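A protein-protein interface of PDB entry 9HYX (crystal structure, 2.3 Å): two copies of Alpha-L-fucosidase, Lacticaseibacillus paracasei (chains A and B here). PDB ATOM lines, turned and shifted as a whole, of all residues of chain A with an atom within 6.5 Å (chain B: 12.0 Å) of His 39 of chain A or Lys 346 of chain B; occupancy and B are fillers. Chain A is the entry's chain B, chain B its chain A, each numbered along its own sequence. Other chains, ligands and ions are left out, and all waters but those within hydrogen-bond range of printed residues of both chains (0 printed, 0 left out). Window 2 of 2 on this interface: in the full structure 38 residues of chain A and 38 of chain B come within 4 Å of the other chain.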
ATOM      1  N   TRP A  33       0.816  17.631  -5.653  1.00  0.00           N
ATOM      2  CA  TRP A  33       1.200  16.650  -6.666  1.00  0.00           C
ATOM      3  C   TRP A  33       2.534  15.975  -6.315  1.00  0.00           C
ATOM      4  O   TRP A  33       3.113  15.321  -7.173  1.00  0.00           O
ATOM      5  CB  TRP A  33       1.324  17.334  -8.033  1.00  0.00           C
ATOM      6  CG  TRP A  33       0.035  17.447  -8.804  1.00  0.00           C
ATOM      7  CD1 TRP A  33      -1.040  18.257  -8.518  1.00  0.00           C
ATOM      8  CD2 TRP A  33      -0.274  16.773 -10.050  1.00  0.00           C
ATOM      9  NE1 TRP A  33      -1.998  18.103  -9.491  1.00  0.00           N
ATOM     10  CE2 TRP A  33      -1.559  17.202 -10.442  1.00  0.00           C
ATOM     11  CE3 TRP A  33       0.426  15.879 -10.868  1.00  0.00           C
ATOM     12  CZ2 TRP A  33      -2.164  16.743 -11.619  1.00  0.00           C
ATOM     13  CZ3 TRP A  33      -0.178  15.406 -12.028  1.00  0.00           C
ATOM     14  CH2 TRP A  33      -1.460  15.828 -12.395  1.00  0.00           C
ATOM     15  N   THR A  34       3.030  16.091  -5.071  1.00  0.00           N
ATOM     16  CA  THR A  34       4.374  15.628  -4.763  1.00  0.00           C
ATOM     17  C   THR A  34       4.621  14.153  -5.162  1.00  0.00           C
ATOM     18  O   THR A  34       5.704  13.794  -5.627  1.00  0.00           O
ATOM     19  CB  THR A  34       4.705  15.908  -3.295  1.00  0.00           C
ATOM     20  OG1 THR A  34       6.037  15.429  -3.134  1.00  0.00           O
ATOM     21  CG2 THR A  34       3.835  15.173  -2.289  1.00  0.00           C
ATOM     22  N   GLU A  35       3.636  13.273  -4.970  1.00  0.00           N
ATOM     23  CA  GLU A  35       3.838  11.851  -5.197  1.00  0.00           C
ATOM     24  C   GLU A  35       4.231  11.579  -6.646  1.00  0.00           C
ATOM     25  O   GLU A  35       5.194  10.867  -6.880  1.00  0.00           O
ATOM     26  CB  GLU A  35       2.674  10.980  -4.716  1.00  0.00           C
ATOM     27  CG  GLU A  35       2.925   9.501  -4.997  1.00  0.00           C
ATOM     28  CD  GLU A  35       1.768   8.594  -4.621  1.00  0.00           C
ATOM     29  OE1 GLU A  35       0.607   9.023  -4.578  1.00  0.00           O
ATOM     30  OE2 GLU A  35       2.052   7.437  -4.297  1.00  0.00           O
ATOM     31  N   LEU A  36       3.501  12.154  -7.602  1.00  0.00           N
ATOM     32  CA  LEU A  36       3.838  11.998  -9.012  1.00  0.00           C
ATOM     33  C   LEU A  36       5.047  12.859  -9.388  1.00  0.00           C
ATOM     34  O   LEU A  36       6.015  12.366  -9.942  1.00  0.00           O
ATOM     35  CB  LEU A  36       2.623  12.295  -9.886  1.00  0.00           C
ATOM     36  CG  LEU A  36       2.805  11.962 -11.378  1.00  0.00           C
ATOM     37  CD1 LEU A  36       1.453  11.579 -11.998  1.00  0.00           C
ATOM     38  CD2 LEU A  36       3.436  13.116 -12.164  1.00  0.00           C
ATOM     39  N   ILE A  37       5.020  14.154  -9.068  1.00  0.00           N
ATOM     40  CA  ILE A  37       5.996  15.071  -9.647  1.00  0.00           C
ATOM     41  C   ILE A  37       7.384  14.825  -9.071  1.00  0.00           C
ATOM     42  O   ILE A  37       8.370  14.975  -9.780  1.00  0.00           O
ATOM     43  CB  ILE A  37       5.547  16.554  -9.596  1.00  0.00           C
ATOM     44  CG1 ILE A  37       4.378  16.748 -10.552  1.00  0.00           C
ATOM     45  CG2 ILE A  37       6.686  17.487  -9.974  1.00  0.00           C
ATOM     46  CD1 ILE A  37       3.672  18.098 -10.458  1.00  0.00           C
ATOM     47  N   HIS A  38       7.472  14.424  -7.803  1.00  0.00           N
ATOM     48  CA  HIS A  38       8.780  14.108  -7.258  1.00  0.00           C
ATOM     49  C   HIS A  38       9.095  12.607  -7.400  1.00  0.00           C
ATOM     50  O   HIS A  38      10.025  12.149  -6.737  1.00  0.00           O
ATOM     51  CB  HIS A  38       8.874  14.501  -5.778  1.00  0.00           C
ATOM     52  CG  HIS A  38       8.813  15.965  -5.544  1.00  0.00           C
ATOM     53  ND1 HIS A  38       7.891  16.557  -4.695  1.00  0.00           N
ATOM     54  CD2 HIS A  38       9.544  16.972  -6.080  1.00  0.00           C
ATOM     55  CE1 HIS A  38       8.113  17.868  -4.676  1.00  0.00           C
ATOM     56  NE2 HIS A  38       9.097  18.143  -5.524  1.00  0.00           N
ATOM     57  N   HIS A  39       8.316  11.865  -8.213  1.00  0.00           N
ATOM     58  CA  HIS A  39       8.536  10.453  -8.538  1.00  0.00           C
ATOM     59  C   HIS A  39       8.865   9.654  -7.281  1.00  0.00           C
ATOM     60  O   HIS A  39       9.899   9.015  -7.205  1.00  0.00           O
ATOM     61  CB  HIS A  39       9.508  10.249  -9.714  1.00  0.00           C
ATOM     62  CG  HIS A  39      10.731  11.101  -9.700  1.00  0.00           C
ATOM     63  ND1 HIS A  39      10.798  12.249 -10.474  1.00  0.00           N
ATOM     64  CD2 HIS A  39      11.945  10.994  -9.094  1.00  0.00           C
ATOM     65  CE1 HIS A  39      11.986  12.836 -10.317  1.00  0.00           C
ATOM     66  NE2 HIS A  39      12.696  12.092  -9.478  1.00  0.00           N
ATOM     67  N   ARG A  40       8.000   9.730  -6.271  1.00  0.00           N
ATOM     68  CA  ARG A  40       8.237   8.995  -5.042  1.00  0.00           C
ATOM     69  C   ARG A  40       7.874   7.514  -5.242  1.00  0.00           C
ATOM     70  O   ARG A  40       7.032   7.155  -6.049  1.00  0.00           O
ATOM     71  CB  ARG A  40       7.363   9.571  -3.927  1.00  0.00           C
ATOM     72  CG  ARG A  40       7.728  11.001  -3.574  1.00  0.00           C
ATOM     73  CD  ARG A  40       6.889  11.524  -2.442  1.00  0.00           C
ATOM     74  NE  ARG A  40       7.106  12.938  -2.154  1.00  0.00           N
ATOM     75  CZ  ARG A  40       8.148  13.454  -1.464  1.00  0.00           C
ATOM     76  NH1 ARG A  40       9.055  12.652  -0.904  1.00  0.00           N
ATOM     77  NH2 ARG A  40       8.242  14.766  -1.262  1.00  0.00           N
ATOM     78  N   ASN A  41       8.499   6.635  -4.460  1.00  0.00           N
ATOM     79  CA  ASN A  41       8.009   5.286  -4.291  1.00  0.00           C
ATOM     80  C   ASN A  41       6.636   5.371  -3.601  1.00  0.00           C
ATOM     81  O   ASN A  41       6.475   5.886  -2.476  1.00  0.00           O
ATOM     82  CB  ASN A  41       9.035   4.478  -3.510  1.00  0.00           C
ATOM     83  CG  ASN A  41       8.510   3.128  -3.115  1.00  0.00           C
ATOM     84  OD1 ASN A  41       7.878   2.991  -2.059  1.00  0.00           O
ATOM     85  ND2 ASN A  41       8.654   2.151  -4.018  1.00  0.00           N
ATOM     86  N   GLN B 342      10.363  29.790 -13.279  1.00  0.00           N
ATOM     87  CA  GLN B 342       9.127  29.089 -12.970  1.00  0.00           C
ATOM     88  C   GLN B 342       9.383  27.740 -12.311  1.00  0.00           C
ATOM     89  O   GLN B 342      10.521  27.310 -12.193  1.00  0.00           O
ATOM     90  CB  GLN B 342       8.363  29.017 -14.284  1.00  0.00           C
ATOM     91  CG  GLN B 342       7.850  30.411 -14.653  1.00  0.00           C
ATOM     92  CD  GLN B 342       7.060  30.352 -15.934  1.00  0.00           C
ATOM     93  OE1 GLN B 342       7.596  30.055 -17.007  1.00  0.00           O
ATOM     94  NE2 GLN B 342       5.758  30.534 -15.797  1.00  0.00           N
ATOM     95  N   VAL B 343       8.301  27.102 -11.861  1.00  0.00           N
ATOM     96  CA  VAL B 343       8.352  25.796 -11.238  1.00  0.00           C
ATOM     97  C   VAL B 343       8.481  24.719 -12.311  1.00  0.00           C
ATOM     98  O   VAL B 343       7.998  24.885 -13.425  1.00  0.00           O
ATOM     99  CB  VAL B 343       7.131  25.603 -10.311  1.00  0.00           C
ATOM    100  CG1 VAL B 343       7.242  24.297  -9.519  1.00  0.00           C
ATOM    101  CG2 VAL B 343       6.970  26.778  -9.353  1.00  0.00           C
ATOM    102  N   VAL B 344       9.209  23.639 -12.005  1.00  0.00           N
ATOM    103  CA  VAL B 344       9.380  22.511 -12.913  1.00  0.00           C
ATOM    104  C   VAL B 344       8.348  21.437 -12.577  1.00  0.00           C
ATOM    105  O   VAL B 344       8.393  20.892 -11.479  1.00  0.00           O
ATOM    106  CB  VAL B 344      10.806  21.960 -12.708  1.00  0.00           C
ATOM    107  CG1 VAL B 344      11.036  20.601 -13.374  1.00  0.00           C
ATOM    108  CG2 VAL B 344      11.857  22.973 -13.149  1.00  0.00           C
ATOM    109  N   GLY B 345       7.451  21.117 -13.525  1.00  0.00           N
ATOM    110  CA  GLY B 345       6.536  19.983 -13.427  1.00  0.00           C
ATOM    111  C   GLY B 345       7.187  18.658 -13.839  1.00  0.00           C
ATOM    112  O   GLY B 345       8.388  18.447 -13.656  1.00  0.00           O
ATOM    113  N   LYS B 346       6.383  17.742 -14.401  1.00  0.00           N
ATOM    114  CA  LYS B 346       6.921  16.449 -14.808  1.00  0.00           C
ATOM    115  C   LYS B 346       6.073  15.863 -15.924  1.00  0.00           C
ATOM    116  O   LYS B 346       4.846  15.980 -15.892  1.00  0.00           O
ATOM    117  CB  LYS B 346       7.008  15.462 -13.643  1.00  0.00           C
ATOM    118  CG  LYS B 346       7.603  14.076 -13.868  1.00  0.00           C
ATOM    119  CD  LYS B 346       9.076  13.770 -13.609  1.00  0.00           C
ATOM    120  CE  LYS B 346       9.284  12.364 -13.126  1.00  0.00           C
ATOM    121  NZ  LYS B 346       8.735  11.342 -14.021  1.00  0.00           N
ATOM    122  N   ASP B 347       6.779  15.279 -16.910  1.00  0.00           N
ATOM    123  CA  ASP B 347       6.188  14.686 -18.106  1.00  0.00           C
ATOM    124  C   ASP B 347       5.184  15.662 -18.728  1.00  0.00           C
ATOM    125  O   ASP B 347       5.574  16.735 -19.180  1.00  0.00           O
ATOM    126  CB  ASP B 347       5.719  13.260 -17.852  1.00  0.00           C
ATOM    127  CG  ASP B 347       6.786  12.289 -17.345  1.00  0.00           C
ATOM    128  OD1 ASP B 347       7.897  12.285 -17.920  1.00  0.00           O
ATOM    129  OD2 ASP B 347       6.497  11.518 -16.399  1.00  0.00           O
ATOM    130  N   ASN B 348       3.889  15.310 -18.713  1.00  0.00           N
ATOM    131  CA  ASN B 348       2.864  16.074 -19.417  1.00  0.00           C
ATOM    132  C   ASN B 348       2.315  17.188 -18.524  1.00  0.00           C
ATOM    133  O   ASN B 348       1.484  17.986 -18.966  1.00  0.00           O
ATOM    134  CB  ASN B 348       1.744  15.188 -19.968  1.00  0.00           C
ATOM    135  CG  ASN B 348       1.011  14.424 -18.882  1.00  0.00           C
ATOM    136  OD1 ASN B 348       1.555  13.478 -18.297  1.00  0.00           O
ATOM    137  ND2 ASN B 348      -0.233  14.799 -18.604  1.00  0.00           N
ATOM    138  N   VAL B 349       2.752  17.232 -17.256  1.00  0.00           N
ATOM    139  CA  VAL B 349       2.424  18.346 -16.363  1.00  0.00           C
ATOM    140  C   VAL B 349       3.497  19.432 -16.511  1.00  0.00           C
ATOM    141  O   VAL B 349       4.607  19.305 -15.993  1.00  0.00           O
ATOM    142  CB  VAL B 349       2.239  17.912 -14.895  1.00  0.00           C
ATOM    143  CG1 VAL B 349       1.585  18.985 -14.042  1.00  0.00           C
ATOM    144  CG2 VAL B 349       1.446  16.615 -14.824  1.00  0.00           C
ATOM    145  N   VAL B 350       3.132  20.492 -17.240  1.00  0.00           N
ATOM    146  CA  VAL B 350       4.045  21.549 -17.641  1.00  0.00           C
ATOM    147  C   VAL B 350       3.733  22.769 -16.776  1.00  0.00           C
ATOM    148  O   VAL B 350       2.618  23.280 -16.831  1.00  0.00           O
ATOM    149  CB  VAL B 350       3.872  21.851 -19.151  1.00  0.00           C
ATOM    150  CG1 VAL B 350       4.609  23.128 -19.594  1.00  0.00           C
ATOM    151  CG2 VAL B 350       4.296  20.678 -20.026  1.00  0.00           C
ATOM    152  N   LEU B 351       4.712  23.218 -15.981  1.00  0.00           N
ATOM    153  CA  LEU B 351       4.504  24.343 -15.073  1.00  0.00           C
ATOM    154  C   LEU B 351       5.240  25.607 -15.547  1.00  0.00           C
ATOM    155  O   LEU B 351       5.020  26.689 -14.988  1.00  0.00           O
ATOM    156  CB  LEU B 351       4.839  23.971 -13.621  1.00  0.00           C
ATOM    157  CG  LEU B 351       4.031  22.809 -13.016  1.00  0.00           C
ATOM    158  CD1 LEU B 351       4.543  22.466 -11.620  1.00  0.00           C
ATOM    159  CD2 LEU B 351       2.522  23.070 -13.003  1.00  0.00           C
ATOM    160  N   GLY B 352       6.047  25.430 -16.581  1.00  0.00           N
ATOM    161  CA  GLY B 352       6.852  26.450 -17.208  1.00  0.00           C
ATOM    162  C   GLY B 352       8.344  26.521 -16.993  1.00  0.00           C
ATOM    163  O   GLY B 352       9.022  27.132 -17.777  1.00  0.00           O
ATOM    164  N   GLY B 353       8.874  25.858 -15.987  1.00  0.00           N
ATOM    165  CA  GLY B 353      10.294  25.903 -15.731  1.00  0.00           C
ATOM    166  C   GLY B 353      11.136  24.854 -16.418  1.00  0.00           C
ATOM    167  O   GLY B 353      12.327  24.853 -16.260  1.00  0.00           O
ATOM    168  N   GLU B 354      10.503  23.953 -17.151  1.00  0.00           N
ATOM    169  CA  GLU B 354      11.139  22.752 -17.685  1.00  0.00           C
ATOM    170  C   GLU B 354      12.261  22.880 -18.714  1.00  0.00           C
ATOM    171  O   GLU B 354      13.235  22.159 -18.649  1.00  0.00           O
ATOM    172  CB  GLU B 354      10.072  21.796 -18.219  1.00  0.00           C
ATOM    173  CG  GLU B 354       9.119  21.281 -17.165  1.00  0.00           C
ATOM    174  CD  GLU B 354       7.945  22.199 -16.922  1.00  0.00           C
ATOM    175  OE1 GLU B 354       7.739  23.131 -17.701  1.00  0.00           O
ATOM    176  OE2 GLU B 354       7.244  21.982 -15.941  1.00  0.00           O
ATOM    177  N   GLY B 355      12.114  23.778 -19.669  1.00  0.00           N
ATOM    178  CA  GLY B 355      13.060  23.884 -20.758  1.00  0.00           C
ATOM    179  C   GLY B 355      14.387  24.462 -20.355  1.00  0.00           C
ATOM    180  O   GLY B 355      14.487  25.076 -19.328  1.00  0.00           O
ATOM    181  N   ASN B 376      19.170  24.496  -3.072  1.00  0.00           N
ATOM    182  CA  ASN B 376      19.252  23.037  -3.101  1.00  0.00           C
ATOM    183  C   ASN B 376      20.610  22.436  -3.452  1.00  0.00           C
ATOM    184  O   ASN B 376      20.770  21.225  -3.462  1.00  0.00           O
ATOM    185  CB  ASN B 376      18.138  22.432  -3.961  1.00  0.00           C
ATOM    186  CG  ASN B 376      18.296  22.742  -5.429  1.00  0.00           C
ATOM    187  OD1 ASN B 376      19.184  23.484  -5.829  1.00  0.00           O
ATOM    188  ND2 ASN B 376      17.425  22.174  -6.240  1.00  0.00           N
ATOM    189  N   GLU B 378      22.015  22.336  -6.295  1.00  0.00           N
ATOM    190  CA  GLU B 378      22.081  21.760  -7.631  1.00  0.00           C
ATOM    191  C   GLU B 378      23.168  22.447  -8.449  1.00  0.00           C
ATOM    192  O   GLU B 378      23.291  23.664  -8.440  1.00  0.00           O
ATOM    193  CB  GLU B 378      20.732  21.852  -8.344  1.00  0.00           C
ATOM    194  CG  GLU B 378      20.762  21.365  -9.784  1.00  0.00           C
ATOM    195  CD  GLU B 378      19.525  21.752 -10.570  1.00  0.00           C
ATOM    196  OE1 GLU B 378      18.721  22.556 -10.073  1.00  0.00           O
ATOM    197  OE2 GLU B 378      19.349  21.244 -11.691  1.00  0.00           O
ATOM    198  N   GLY B 397      14.541  25.673 -13.381  1.00  0.00           N
ATOM    199  CA  GLY B 397      13.406  26.180 -12.645  1.00  0.00           C
ATOM    200  C   GLY B 397      13.329  25.548 -11.255  1.00  0.00           C
ATOM    201  O   GLY B 397      14.132  24.688 -10.907  1.00  0.00           O
ATOM    202  N   TYR B 398      12.376  26.017 -10.437  1.00  0.00           N
ATOM    203  CA  TYR B 398      12.299  25.584  -9.051  1.00  0.00           C
ATOM    204  C   TYR B 398      11.811  24.138  -8.985  1.00  0.00           C
ATOM    205  O   TYR B 398      10.923  23.725  -9.728  1.00  0.00           O
ATOM    206  CB  TYR B 398      11.262  26.446  -8.320  1.00  0.00           C
ATOM    207  CG  TYR B 398      11.635  27.923  -8.312  1.00  0.00           C
ATOM    208  CD1 TYR B 398      12.758  28.358  -7.612  1.00  0.00           C
ATOM    209  CD2 TYR B 398      10.875  28.872  -8.999  1.00  0.00           C
ATOM    210  CE1 TYR B 398      13.116  29.688  -7.578  1.00  0.00           C
ATOM    211  CE2 TYR B 398      11.221  30.215  -8.983  1.00  0.00           C
ATOM    212  CZ  TYR B 398      12.338  30.612  -8.252  1.00  0.00           C
ATOM    213  OH  TYR B 398      12.746  31.909  -8.188  1.00  0.00           O
ATOM    214  N   PRO B 399      12.324  23.340  -8.030  1.00  0.00           N
ATOM    215  CA  PRO B 399      11.686  22.068  -7.706  1.00  0.00           C
ATOM    216  C   PRO B 399      10.226  22.288  -7.340  1.00  0.00           C
ATOM    217  O   PRO B 399       9.913  23.238  -6.615  1.00  0.00           O
ATOM    218  CB  PRO B 399      12.456  21.518  -6.494  1.00  0.00           C
ATOM    219  CG  PRO B 399      13.721  22.355  -6.450  1.00  0.00           C
ATOM    220  CD  PRO B 399      13.458  23.668  -7.157  1.00  0.00           C
ATOM    221  N   TYR B 400       9.349  21.403  -7.829  1.00  0.00           N
ATOM    222  CA  TYR B 400       7.937  21.474  -7.501  1.00  0.00           C
ATOM    223  C   TYR B 400       7.828  21.605  -5.988  1.00  0.00           C
ATOM    224  O   TYR B 400       8.578  20.971  -5.256  1.00  0.00           O
ATOM    225  CB  TYR B 400       7.197  20.251  -8.051  1.00  0.00           C
ATOM    226  CG  TYR B 400       5.728  20.241  -7.648  1.00  0.00           C
ATOM    227  CD1 TYR B 400       4.787  21.075  -8.281  1.00  0.00           C
ATOM    228  CD2 TYR B 400       5.302  19.446  -6.601  1.00  0.00           C
ATOM    229  CE1 TYR B 400       3.462  21.095  -7.889  1.00  0.00           C
ATOM    230  CE2 TYR B 400       3.965  19.404  -6.239  1.00  0.00           C
ATOM    231  CZ  TYR B 400       3.062  20.275  -6.841  1.00  0.00           C
ATOM    232  OH  TYR B 400       1.760  20.263  -6.426  1.00  0.00           O
ATOM    233  N   GLY B 401       6.930  22.479  -5.528  1.00  0.00           N
ATOM    234  CA  GLY B 401       6.736  22.674  -4.100  1.00  0.00           C
ATOM    235  C   GLY B 401       7.527  23.858  -3.567  1.00  0.00           C
ATOM    236  O   GLY B 401       7.461  24.166  -2.362  1.00  0.00           O
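OH of Tyr 400 of chain B is in hydrogen-bond range of N of Trp 33 of chain A.
A ring nitrogen (NE2) of His 38 of chain A is in hydrogen-bond range of the backbone carbonyl oxygen (O) of Tyr 400 of chain B (2.9 Å).
Of the printed residues of chain B, His 39 of chain A touches Lys 346.
Printed residues of chain A within 4 Å of Lys 346 of chain B: His 39 (3.1 Å).
No residue of chain B comes within 4 Å of Leu 36 of chain A.
Of chain B, only Tyr 400 (3.4 Å) comes within 4 Å of Ile 37 of chain A.
His 38 of chain A touches just one residue of chain B: Tyr 400.
Of the printed residues of chain A, Tyr 400 of chain B touches Trp 33, Thr 34, Ile 37 and His 38.
Of the printed residues of chain B, Thr 34 of chain A touches Tyr 400 (3.6 Å).
Printed residues of chain B within 4 Å of Trp 33 of chain A: Val 349 and Tyr 400.
Printed residues of chain A within 4 Å of Val 349 of chain B: Trp 33 (3.5 Å).
Val 350 of chain B touches none of the printed residues of chain A.
The nearest printed residue of chain B that does not touch Thr 34 of chain A is Gly 401 of chain B (7.1 Å).
No position is printed for both chains.
CG2 of Val 349 of chain B touches CZ3 of Trp 33 of chain A, at 3.5 Å.
Thr 34 of chain A touches Tyr 400 of chain B (N to CE2, 3.6 Å).
Tyr 400 of chain B touches Ile 37 of chain A.
His 39 of chain A touches Lys 346 of chain B (ND1 to CE, 3.1 Å).
Printed residues of chain A that touch a printed residue of chain B: Trp 33, Thr 34, Ile 37, His 38 and His 39.
Hydrophobic or aromatic side chains of chain A within 4 Å of the printed part of chain B: Trp 33, Ile 37, His 38 and His 39.
Along chain A the printed residues that touch a printed residue of chain B span positions 33 to 39.
Of the 21 printed residues of chain B, 3 touch a printed residue of chain A.
Printed residues of chain B that touch a printed residue of chain A: Lys 346, Val 349 and Tyr 400.
Among the printed residues, 6 pairs touch across the chains.
The side-chain amino group of Lys 346 of chain B lies within salt-bridge range of the side-chain carboxylate of Asp 347 of chain B (3.3 Å).
The side-chain hydroxyl of Thr 34 of chain A sits at hydrogen-bond distance from a ring nitrogen (ND1) of His 38 of chain A, at 2.7 Å.
The side-chain hydroxyl (OG1) of Thr 34 of chain A sits at hydrogen-bond distance from the guanidinium group (NE) of Arg 40 of chain A (2.9 Å).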
